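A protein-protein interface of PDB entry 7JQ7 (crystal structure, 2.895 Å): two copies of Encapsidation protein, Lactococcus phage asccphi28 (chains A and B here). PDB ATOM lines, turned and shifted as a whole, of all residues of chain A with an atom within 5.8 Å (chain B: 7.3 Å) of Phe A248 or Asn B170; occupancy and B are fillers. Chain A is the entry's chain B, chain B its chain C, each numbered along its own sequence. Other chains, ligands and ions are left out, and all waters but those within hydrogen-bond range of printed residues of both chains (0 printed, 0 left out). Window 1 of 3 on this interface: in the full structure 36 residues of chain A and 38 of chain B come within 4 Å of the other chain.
The side-chain amide nitrogen (ND2) of Asn B163 lies within hydrogen-bond range of the side-chain carboxylate (OD2) of Asp A247 (2.4 Å).
The side-chain amino group (NZ) of Lys A252 lies within salt-bridge range of the side-chain carboxylate (OE2) of Glu B173 (2.9 Å).
No position is printed for both chains.
Of the printed residues of chain B, Phe A248 touches Thr B166 (3.7 Å), Leu B169 (3.4 Å), Asn B170 (2.9 Å) and Glu B173 (3.9 Å).
Of chain A, only Phe A248 comes within 4 Å of Asn B170.
Printed residues of chain A within 4 Å of Asn B163: Asp A247.
Of the printed residues of chain B, Gly A242 touches Leu B169.
Printed residues of chain A within 4 Å of Glu B173: Phe A248 (3.9 Å) and Lys A252 (2.9 Å).
The nearest residue of chain B that does not touch Phe A248 is Phe B165 (5.7 Å).
The nearest residue of chain A that does not touch Asn B170 is Ser A251 (4.6 Å).
The nearest printed residue of chain A that does not touch Thr B166 is Ser A251 (4.9 Å).
Leu B169 touches Gly A242 (CD1 to CA, 3.8 Å).
Asn A245 touches Phe B165.
OD2 of Asp A247 touches OG1 of Thr B166 (3.6 Å).
Phe A248 touches Thr B166 (N to OG1, 3.7 Å).
Phe A248 touches Leu B169.
Phe A248 touches Asn B170 (CE1 to OD1, 2.9 Å).
Phe A248 touches Glu B173 (CZ to OE1, 3.9 Å).
The backbone carbonyl oxygen (O) of Asn A245 sits at hydrogen-bond distance from the side-chain hydroxyl (OG) of Ser A249 (2.5 Å).
The backbone carbonyl oxygen (O) of Asn B170 lies within hydrogen-bond range of the side-chain hydroxyl (OG1) of Thr B174, 3.1 Å away.
The side-chain amide oxygen (OD1) of Asn B163 is in hydrogen-bond range of the side-chain hydroxyl (OG1) of Thr B166 (3.0 Å).
The backbone carbonyl oxygen (O) of Gly A242 lies within hydrogen-bond range of the side-chain hydroxyl (OG) of Ser A249, 2.8 Å away.
Of the 18 printed residues of chain B, 6 touch a printed residue of chain A.
Hydrophobic or aromatic side chains of chain B that line the printed part of chain A: Phe B165 and Leu B169.
Of the 10 printed residues of chain A, 5 touch a printed residue of chain B.
Printed residues of chain A that touch a printed residue of chain B: Gly A242, Asn A245, Asp A247, Phe A248 and Lys A252.
Among the printed residues, 9 pairs touch across the chains.
Among the printed residues, Asp or Glu carboxylates within 4 Å of a Lys or Arg side-chain nitrogen of the other chain: Lys A252 with Glu B173 (2.9 Å).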
ATOM      1  N   GLY A 242      -5.412  -0.431   0.744  1.00  0.00           N
ATOM      2  CA  GLY A 242      -5.956  -0.136   2.056  1.00  0.00           C
ATOM      3  C   GLY A 242      -4.901  -0.206   3.141  1.00  0.00           C
ATOM      4  O   GLY A 242      -4.919   0.581   4.090  1.00  0.00           O
ATOM      5  N   ALA A 243      -3.973  -1.157   3.025  1.00  0.00           N
ATOM      6  CA  ALA A 243      -2.924  -1.286   4.026  1.00  0.00           C
ATOM      7  C   ALA A 243      -2.044  -0.047   4.062  1.00  0.00           C
ATOM      8  O   ALA A 243      -1.519   0.311   5.122  1.00  0.00           O
ATOM      9  CB  ALA A 243      -2.079  -2.525   3.739  1.00  0.00           C
ATOM     10  N   ASN A 245      -3.028   2.983   3.697  1.00  0.00           N
ATOM     11  CA  ASN A 245      -3.756   4.100   4.286  1.00  0.00           C
ATOM     12  C   ASN A 245      -3.983   3.836   5.767  1.00  0.00           C
ATOM     13  O   ASN A 245      -4.687   2.892   6.141  1.00  0.00           O
ATOM     14  CB  ASN A 245      -5.082   4.328   3.569  1.00  0.00           C
ATOM     15  CG  ASN A 245      -4.897   4.937   2.206  1.00  0.00           C
ATOM     16  OD1 ASN A 245      -5.067   6.146   2.022  1.00  0.00           O
ATOM     17  ND2 ASN A 245      -4.496   4.115   1.245  1.00  0.00           N
ATOM     18  N   ARG A 246      -3.382   4.681   6.603  1.00  0.00           N
ATOM     19  CA  ARG A 246      -3.482   4.526   8.048  1.00  0.00           C
ATOM     20  C   ARG A 246      -4.936   4.565   8.503  1.00  0.00           C
ATOM     21  O   ARG A 246      -5.427   3.631   9.150  1.00  0.00           O
ATOM     22  CB  ARG A 246      -2.664   5.629   8.726  1.00  0.00           C
ATOM     23  CG  ARG A 246      -2.685   5.602  10.235  1.00  0.00           C
ATOM     24  CD  ARG A 246      -1.767   4.528  10.778  1.00  0.00           C
ATOM     25  NE  ARG A 246      -1.851   4.455  12.233  1.00  0.00           N
ATOM     26  CZ  ARG A 246      -1.074   3.692  12.993  1.00  0.00           C
ATOM     27  NH1 ARG A 246      -0.137   2.936  12.441  1.00  0.00           N
ATOM     28  NH2 ARG A 246      -1.236   3.693  14.307  1.00  0.00           N
ATOM     29  N   ASP A 247      -5.645   5.645   8.161  1.00  0.00           N
ATOM     30  CA  ASP A 247      -6.986   5.859   8.692  1.00  0.00           C
ATOM     31  C   ASP A 247      -7.892   4.669   8.407  1.00  0.00           C
ATOM     32  O   ASP A 247      -8.538   4.132   9.314  1.00  0.00           O
ATOM     33  CB  ASP A 247      -7.576   7.134   8.094  1.00  0.00           C
ATOM     34  CG  ASP A 247      -8.894   7.514   8.725  1.00  0.00           C
ATOM     35  OD1 ASP A 247      -9.402   6.738   9.561  1.00  0.00           O
ATOM     36  OD2 ASP A 247      -9.426   8.587   8.381  1.00  0.00           O
ATOM     37  N   PHE A 248      -7.944   4.232   7.149  1.00  0.00           N
ATOM     38  CA  PHE A 248      -8.768   3.077   6.801  1.00  0.00           C
ATOM     39  C   PHE A 248      -8.341   1.845   7.587  1.00  0.00           C
ATOM     40  O   PHE A 248      -9.186   1.074   8.058  1.00  0.00           O
ATOM     41  CB  PHE A 248      -8.687   2.827   5.290  1.00  0.00           C
ATOM     42  CG  PHE A 248      -9.300   1.525   4.846  1.00  0.00           C
ATOM     43  CD1 PHE A 248     -10.669   1.397   4.698  1.00  0.00           C
ATOM     44  CD2 PHE A 248      -8.498   0.434   4.557  1.00  0.00           C
ATOM     45  CE1 PHE A 248     -11.228   0.191   4.278  1.00  0.00           C
ATOM     46  CE2 PHE A 248      -9.048  -0.767   4.142  1.00  0.00           C
ATOM     47  CZ  PHE A 248     -10.413  -0.889   4.003  1.00  0.00           C
ATOM     48  N   SER A 249      -7.033   1.651   7.755  1.00  0.00           N
ATOM     49  CA  SER A 249      -6.553   0.452   8.427  1.00  0.00           C
ATOM     50  C   SER A 249      -6.935   0.448   9.902  1.00  0.00           C
ATOM     51  O   SER A 249      -7.500  -0.533  10.396  1.00  0.00           O
ATOM     52  CB  SER A 249      -5.040   0.354   8.256  1.00  0.00           C
ATOM     53  OG  SER A 249      -4.684   0.543   6.895  1.00  0.00           O
ATOM     54  N   ASN A 250      -6.666   1.546  10.619  1.00  0.00           N
ATOM     55  CA  ASN A 250      -7.062   1.599  12.023  1.00  0.00           C
ATOM     56  C   ASN A 250      -8.575   1.495  12.155  1.00  0.00           C
ATOM     57  O   ASN A 250      -9.081   0.921  13.126  1.00  0.00           O
ATOM     58  CB  ASN A 250      -6.554   2.875  12.692  1.00  0.00           C
ATOM     59  CG  ASN A 250      -5.197   2.683  13.353  1.00  0.00           C
ATOM     60  OD1 ASN A 250      -4.711   1.558  13.494  1.00  0.00           O
ATOM     61  ND2 ASN A 250      -4.583   3.783  13.773  1.00  0.00           N
ATOM     62  N   SER A 251      -9.310   2.038  11.183  1.00  0.00           N
ATOM     63  CA  SER A 251     -10.765   2.023  11.231  1.00  0.00           C
ATOM     64  C   SER A 251     -11.309   0.611  11.399  1.00  0.00           C
ATOM     65  O   SER A 251     -12.438   0.443  11.869  1.00  0.00           O
ATOM     66  CB  SER A 251     -11.318   2.668   9.959  1.00  0.00           C
ATOM     67  OG  SER A 251     -12.729   2.786  10.004  1.00  0.00           O
ATOM     68  N   LYS A 252     -10.535  -0.409  11.030  1.00  0.00           N
ATOM     69  CA  LYS A 252     -11.012  -1.775  11.185  1.00  0.00           C
ATOM     70  C   LYS A 252     -11.140  -2.172  12.651  1.00  0.00           C
ATOM     71  O   LYS A 252     -12.014  -2.976  12.995  1.00  0.00           O
ATOM     72  CB  LYS A 252     -10.071  -2.746  10.479  1.00  0.00           C
ATOM     73  CG  LYS A 252      -9.926  -2.525   8.987  1.00  0.00           C
ATOM     74  CD  LYS A 252      -8.921  -3.510   8.404  1.00  0.00           C
ATOM     75  CE  LYS A 252      -8.857  -3.425   6.890  1.00  0.00           C
ATOM     76  NZ  LYS A 252     -10.112  -3.910   6.243  1.00  0.00           N
ATOM     77  N   ALA B 129     -22.836   6.293   1.223  1.00  0.00           N
ATOM     78  CA  ALA B 129     -22.177   5.020   1.490  1.00  0.00           C
ATOM     79  C   ALA B 129     -22.220   4.639   2.967  1.00  0.00           C
ATOM     80  O   ALA B 129     -22.282   3.449   3.292  1.00  0.00           O
ATOM     81  CB  ALA B 129     -20.730   5.076   0.999  1.00  0.00           C
ATOM     82  N   VAL B 132     -24.952   2.273   3.812  1.00  0.00           N
ATOM     83  CA  VAL B 132     -25.031   1.005   3.100  1.00  0.00           C
ATOM     84  C   VAL B 132     -24.094  -0.038   3.708  1.00  0.00           C
ATOM     85  O   VAL B 132     -23.743  -1.014   3.043  1.00  0.00           O
ATOM     86  CB  VAL B 132     -24.756   1.181   1.593  1.00  0.00           C
ATOM     87  CG1 VAL B 132     -25.590   2.332   1.018  1.00  0.00           C
ATOM     88  CG2 VAL B 132     -23.268   1.412   1.309  1.00  0.00           C
ATOM     89  N   LYS B 133     -23.679   0.153   4.961  1.00  0.00           N
ATOM     90  CA  LYS B 133     -22.699  -0.741   5.568  1.00  0.00           C
ATOM     91  C   LYS B 133     -23.088  -2.205   5.377  1.00  0.00           C
ATOM     92  O   LYS B 133     -22.296  -3.014   4.880  1.00  0.00           O
ATOM     93  CB  LYS B 133     -22.546  -0.407   7.055  1.00  0.00           C
ATOM     94  N   ASN B 163     -12.895  12.742   4.801  1.00  0.00           N
ATOM     95  CA  ASN B 163     -12.175  11.473   4.809  1.00  0.00           C
ATOM     96  C   ASN B 163     -12.625  10.598   3.649  1.00  0.00           C
ATOM     97  O   ASN B 163     -12.911   9.410   3.807  1.00  0.00           O
ATOM     98  CB  ASN B 163     -12.363  10.734   6.127  1.00  0.00           C
ATOM     99  CG  ASN B 163     -11.267   9.719   6.379  1.00  0.00           C
ATOM    100  OD1 ASN B 163     -10.192   9.769   5.766  1.00  0.00           O
ATOM    101  ND2 ASN B 163     -11.543   8.766   7.263  1.00  0.00           N
ATOM    102  N   GLU B 164     -12.683  11.204   2.463  1.00  0.00           N
ATOM    103  CA  GLU B 164     -13.334  10.554   1.331  1.00  0.00           C
ATOM    104  C   GLU B 164     -12.672   9.224   0.994  1.00  0.00           C
ATOM    105  O   GLU B 164     -13.343   8.192   0.901  1.00  0.00           O
ATOM    106  CB  GLU B 164     -13.327  11.492   0.128  1.00  0.00           C
ATOM    107  CG  GLU B 164     -13.706  10.827  -1.169  1.00  0.00           C
ATOM    108  CD  GLU B 164     -14.201  11.815  -2.195  1.00  0.00           C
ATOM    109  OE1 GLU B 164     -15.056  12.655  -1.845  1.00  0.00           O
ATOM    110  OE2 GLU B 164     -13.738  11.765  -3.353  1.00  0.00           O
ATOM    111  N   PHE B 165     -11.348   9.219   0.825  1.00  0.00           N
ATOM    112  CA  PHE B 165     -10.685   8.005   0.372  1.00  0.00           C
ATOM    113  C   PHE B 165     -10.898   6.850   1.341  1.00  0.00           C
ATOM    114  O   PHE B 165     -10.911   5.689   0.924  1.00  0.00           O
ATOM    115  CB  PHE B 165      -9.194   8.244   0.165  1.00  0.00           C
ATOM    116  CG  PHE B 165      -8.548   7.215  -0.704  1.00  0.00           C
ATOM    117  CD1 PHE B 165      -8.667   7.285  -2.082  1.00  0.00           C
ATOM    118  CD2 PHE B 165      -7.831   6.172  -0.148  1.00  0.00           C
ATOM    119  CE1 PHE B 165      -8.079   6.334  -2.890  1.00  0.00           C
ATOM    120  CE2 PHE B 165      -7.237   5.217  -0.948  1.00  0.00           C
ATOM    121  CZ  PHE B 165      -7.361   5.296  -2.321  1.00  0.00           C
ATOM    122  N   THR B 166     -11.036   7.137   2.635  1.00  0.00           N
ATOM    123  CA  THR B 166     -11.366   6.076   3.579  1.00  0.00           C
ATOM    124  C   THR B 166     -12.788   5.578   3.347  1.00  0.00           C
ATOM    125  O   THR B 166     -13.066   4.381   3.485  1.00  0.00           O
ATOM    126  CB  THR B 166     -11.196   6.563   5.018  1.00  0.00           C
ATOM    127  OG1 THR B 166      -9.814   6.839   5.280  1.00  0.00           O
ATOM    128  CG2 THR B 166     -11.680   5.510   5.998  1.00  0.00           C
ATOM    129  N   VAL B 167     -13.704   6.485   2.996  1.00  0.00           N
ATOM    130  CA  VAL B 167     -15.062   6.073   2.646  1.00  0.00           C
ATOM    131  C   VAL B 167     -15.039   5.136   1.443  1.00  0.00           C
ATOM    132  O   VAL B 167     -15.668   4.071   1.448  1.00  0.00           O
ATOM    133  CB  VAL B 167     -15.941   7.306   2.364  1.00  0.00           C
ATOM    134  CG1 VAL B 167     -17.325   6.874   1.895  1.00  0.00           C
ATOM    135  CG2 VAL B 167     -16.043   8.193   3.584  1.00  0.00           C
ATOM    136  N   LEU B 168     -14.299   5.514   0.399  1.00  0.00           N
ATOM    137  CA  LEU B 168     -14.239   4.699  -0.810  1.00  0.00           C
ATOM    138  C   LEU B 168     -13.695   3.304  -0.517  1.00  0.00           C
ATOM    139  O   LEU B 168     -14.254   2.302  -0.972  1.00  0.00           O
ATOM    140  CB  LEU B 168     -13.398   5.406  -1.870  1.00  0.00           C
ATOM    141  CG  LEU B 168     -13.274   4.663  -3.200  1.00  0.00           C
ATOM    142  CD1 LEU B 168     -14.648   4.502  -3.839  1.00  0.00           C
ATOM    143  CD2 LEU B 168     -12.326   5.404  -4.136  1.00  0.00           C
ATOM    144  N   LEU B 169     -12.591   3.212   0.221  1.00  0.00           N
ATOM    145  CA  LEU B 169     -12.046   1.895   0.529  1.00  0.00           C
ATOM    146  C   LEU B 169     -13.076   1.024   1.238  1.00  0.00           C
ATOM    147  O   LEU B 169     -13.219  -0.161   0.921  1.00  0.00           O
ATOM    148  CB  LEU B 169     -10.781   2.025   1.374  1.00  0.00           C
ATOM    149  CG  LEU B 169      -9.521   2.515   0.664  1.00  0.00           C
ATOM    150  CD1 LEU B 169      -8.422   2.701   1.683  1.00  0.00           C
ATOM    151  CD2 LEU B 169      -9.068   1.544  -0.409  1.00  0.00           C
ATOM    152  N   ASN B 170     -13.812   1.594   2.194  1.00  0.00           N
ATOM    153  CA  ASN B 170     -14.877   0.844   2.858  1.00  0.00           C
ATOM    154  C   ASN B 170     -15.893   0.323   1.849  1.00  0.00           C
ATOM    155  O   ASN B 170     -16.415  -0.789   1.993  1.00  0.00           O
ATOM    156  CB  ASN B 170     -15.543   1.738   3.900  1.00  0.00           C
ATOM    157  CG  ASN B 170     -14.742   1.836   5.186  1.00  0.00           C
ATOM    158  OD1 ASN B 170     -13.751   1.132   5.374  1.00  0.00           O
ATOM    159  ND2 ASN B 170     -15.113   2.787   6.034  1.00  0.00           N
ATOM    160  N   LEU B 171     -16.190   1.117   0.821  1.00  0.00           N
ATOM    161  CA  LEU B 171     -17.128   0.671  -0.201  1.00  0.00           C
ATOM    162  C   LEU B 171     -16.530  -0.448  -1.042  1.00  0.00           C
ATOM    163  O   LEU B 171     -17.224  -1.411  -1.378  1.00  0.00           O
ATOM    164  CB  LEU B 171     -17.542   1.846  -1.087  1.00  0.00           C
ATOM    165  CG  LEU B 171     -18.581   1.563  -2.170  1.00  0.00           C
ATOM    166  CD1 LEU B 171     -19.869   1.019  -1.580  1.00  0.00           C
ATOM    167  CD2 LEU B 171     -18.854   2.840  -2.954  1.00  0.00           C
ATOM    168  N   ILE B 172     -15.243  -0.351  -1.381  1.00  0.00           N
ATOM    169  CA  ILE B 172     -14.607  -1.414  -2.152  1.00  0.00           C
ATOM    170  C   ILE B 172     -14.722  -2.742  -1.412  1.00  0.00           C
ATOM    171  O   ILE B 172     -15.113  -3.764  -1.989  1.00  0.00           O
ATOM    172  CB  ILE B 172     -13.138  -1.064  -2.449  1.00  0.00           C
ATOM    173  CG1 ILE B 172     -13.039   0.263  -3.206  1.00  0.00           C
ATOM    174  CG2 ILE B 172     -12.504  -2.192  -3.253  1.00  0.00           C
ATOM    175  CD1 ILE B 172     -11.611   0.706  -3.537  1.00  0.00           C
ATOM    176  N   GLU B 173     -14.378  -2.748  -0.121  1.00  0.00           N
ATOM    177  CA  GLU B 173     -14.429  -3.983   0.660  1.00  0.00           C
ATOM    178  C   GLU B 173     -15.848  -4.531   0.736  1.00  0.00           C
ATOM    179  O   GLU B 173     -16.054  -5.748   0.676  1.00  0.00           O
ATOM    180  CB  GLU B 173     -13.875  -3.740   2.063  1.00  0.00           C
ATOM    181  CG  GLU B 173     -13.241  -4.964   2.707  1.00  0.00           C
ATOM    182  CD  GLU B 173     -12.710  -4.682   4.106  1.00  0.00           C
ATOM    183  OE1 GLU B 173     -13.055  -3.626   4.680  1.00  0.00           O
ATOM    184  OE2 GLU B 173     -11.918  -5.506   4.615  1.00  0.00           O
ATOM    185  N   THR B 174     -16.842  -3.653   0.878  1.00  0.00           N
ATOM    186  CA  THR B 174     -18.224  -4.114   0.953  1.00  0.00           C
ATOM    187  C   THR B 174     -18.669  -4.701  -0.380  1.00  0.00           C
ATOM    188  O   THR B 174     -19.255  -5.788  -0.428  1.00  0.00           O
ATOM    189  CB  THR B 174     -19.135  -2.963   1.374  1.00  0.00           C
ATOM    190  OG1 THR B 174     -18.821  -2.571   2.718  1.00  0.00           O
ATOM    191  CG2 THR B 174     -20.591  -3.371   1.287  1.00  0.00           C
ATOM    192  N   ILE B 175     -18.362  -4.011  -1.478  1.00  0.00           N
ATOM    193  CA  ILE B 175     -18.750  -4.493  -2.798  1.00  0.00           C
ATOM    194  C   ILE B 175     -17.940  -5.725  -3.168  1.00  0.00           C
ATOM    195  O   ILE B 175     -18.448  -6.650  -3.809  1.00  0.00           O
ATOM    196  CB  ILE B 175     -18.591  -3.370  -3.841  1.00  0.00           C
ATOM    197  CG1 ILE B 175     -19.563  -2.226  -3.539  1.00  0.00           C
ATOM    198  CG2 ILE B 175     -18.795  -3.921  -5.236  1.00  0.00           C
ATOM    199  CD1 ILE B 175     -19.424  -1.024  -4.452  1.00  0.00           C
ATOM    200  N   LYS B 176     -16.668  -5.752  -2.777  1.00  0.00           N
ATOM    201  CA  LYS B 176     -15.738  -6.830  -3.105  1.00  0.00           C
ATOM    202  C   LYS B 176     -15.492  -7.643  -1.842  1.00  0.00           C
ATOM    203  O   LYS B 176     -14.802  -7.182  -0.926  1.00  0.00           O
ATOM    204  CB  LYS B 176     -14.434  -6.254  -3.654  1.00  0.00           C
ATOM    205  CG  LYS B 176     -13.287  -7.240  -3.758  1.00  0.00           C
ATOM    206  CD  LYS B 176     -11.968  -6.484  -3.921  1.00  0.00           C
ATOM    207  CE  LYS B 176     -10.793  -7.431  -4.085  1.00  0.00           C
ATOM    208  NZ  LYS B 176     -10.615  -8.301  -2.884  1.00  0.00           N
ATOM    209  N   TYR B 277       1.777  10.428  13.130  1.00  0.00           N
ATOM    210  CA  TYR B 277       0.894   9.916  12.086  1.00  0.00           C
ATOM    211  C   TYR B 277       1.640   8.941  11.192  1.00  0.00           C
ATOM    212  O   TYR B 277       2.677   9.291  10.620  1.00  0.00           O
ATOM    213  CB  TYR B 277       0.325  11.059  11.245  1.00  0.00           C
ATOM    214  CG  TYR B 277      -0.836  10.657  10.381  1.00  0.00           C
ATOM    215  CD1 TYR B 277      -2.084  10.417  10.933  1.00  0.00           C
ATOM    216  CD2 TYR B 277      -0.683  10.504   9.008  1.00  0.00           C
ATOM    217  CE1 TYR B 277      -3.158  10.041  10.141  1.00  0.00           C
ATOM    218  CE2 TYR B 277      -1.747  10.133   8.206  1.00  0.00           C
ATOM    219  CZ  TYR B 277      -2.983   9.900   8.778  1.00  0.00           C
ATOM    220  OH  TYR B 277      -4.045   9.528   7.987  1.00  0.00           O
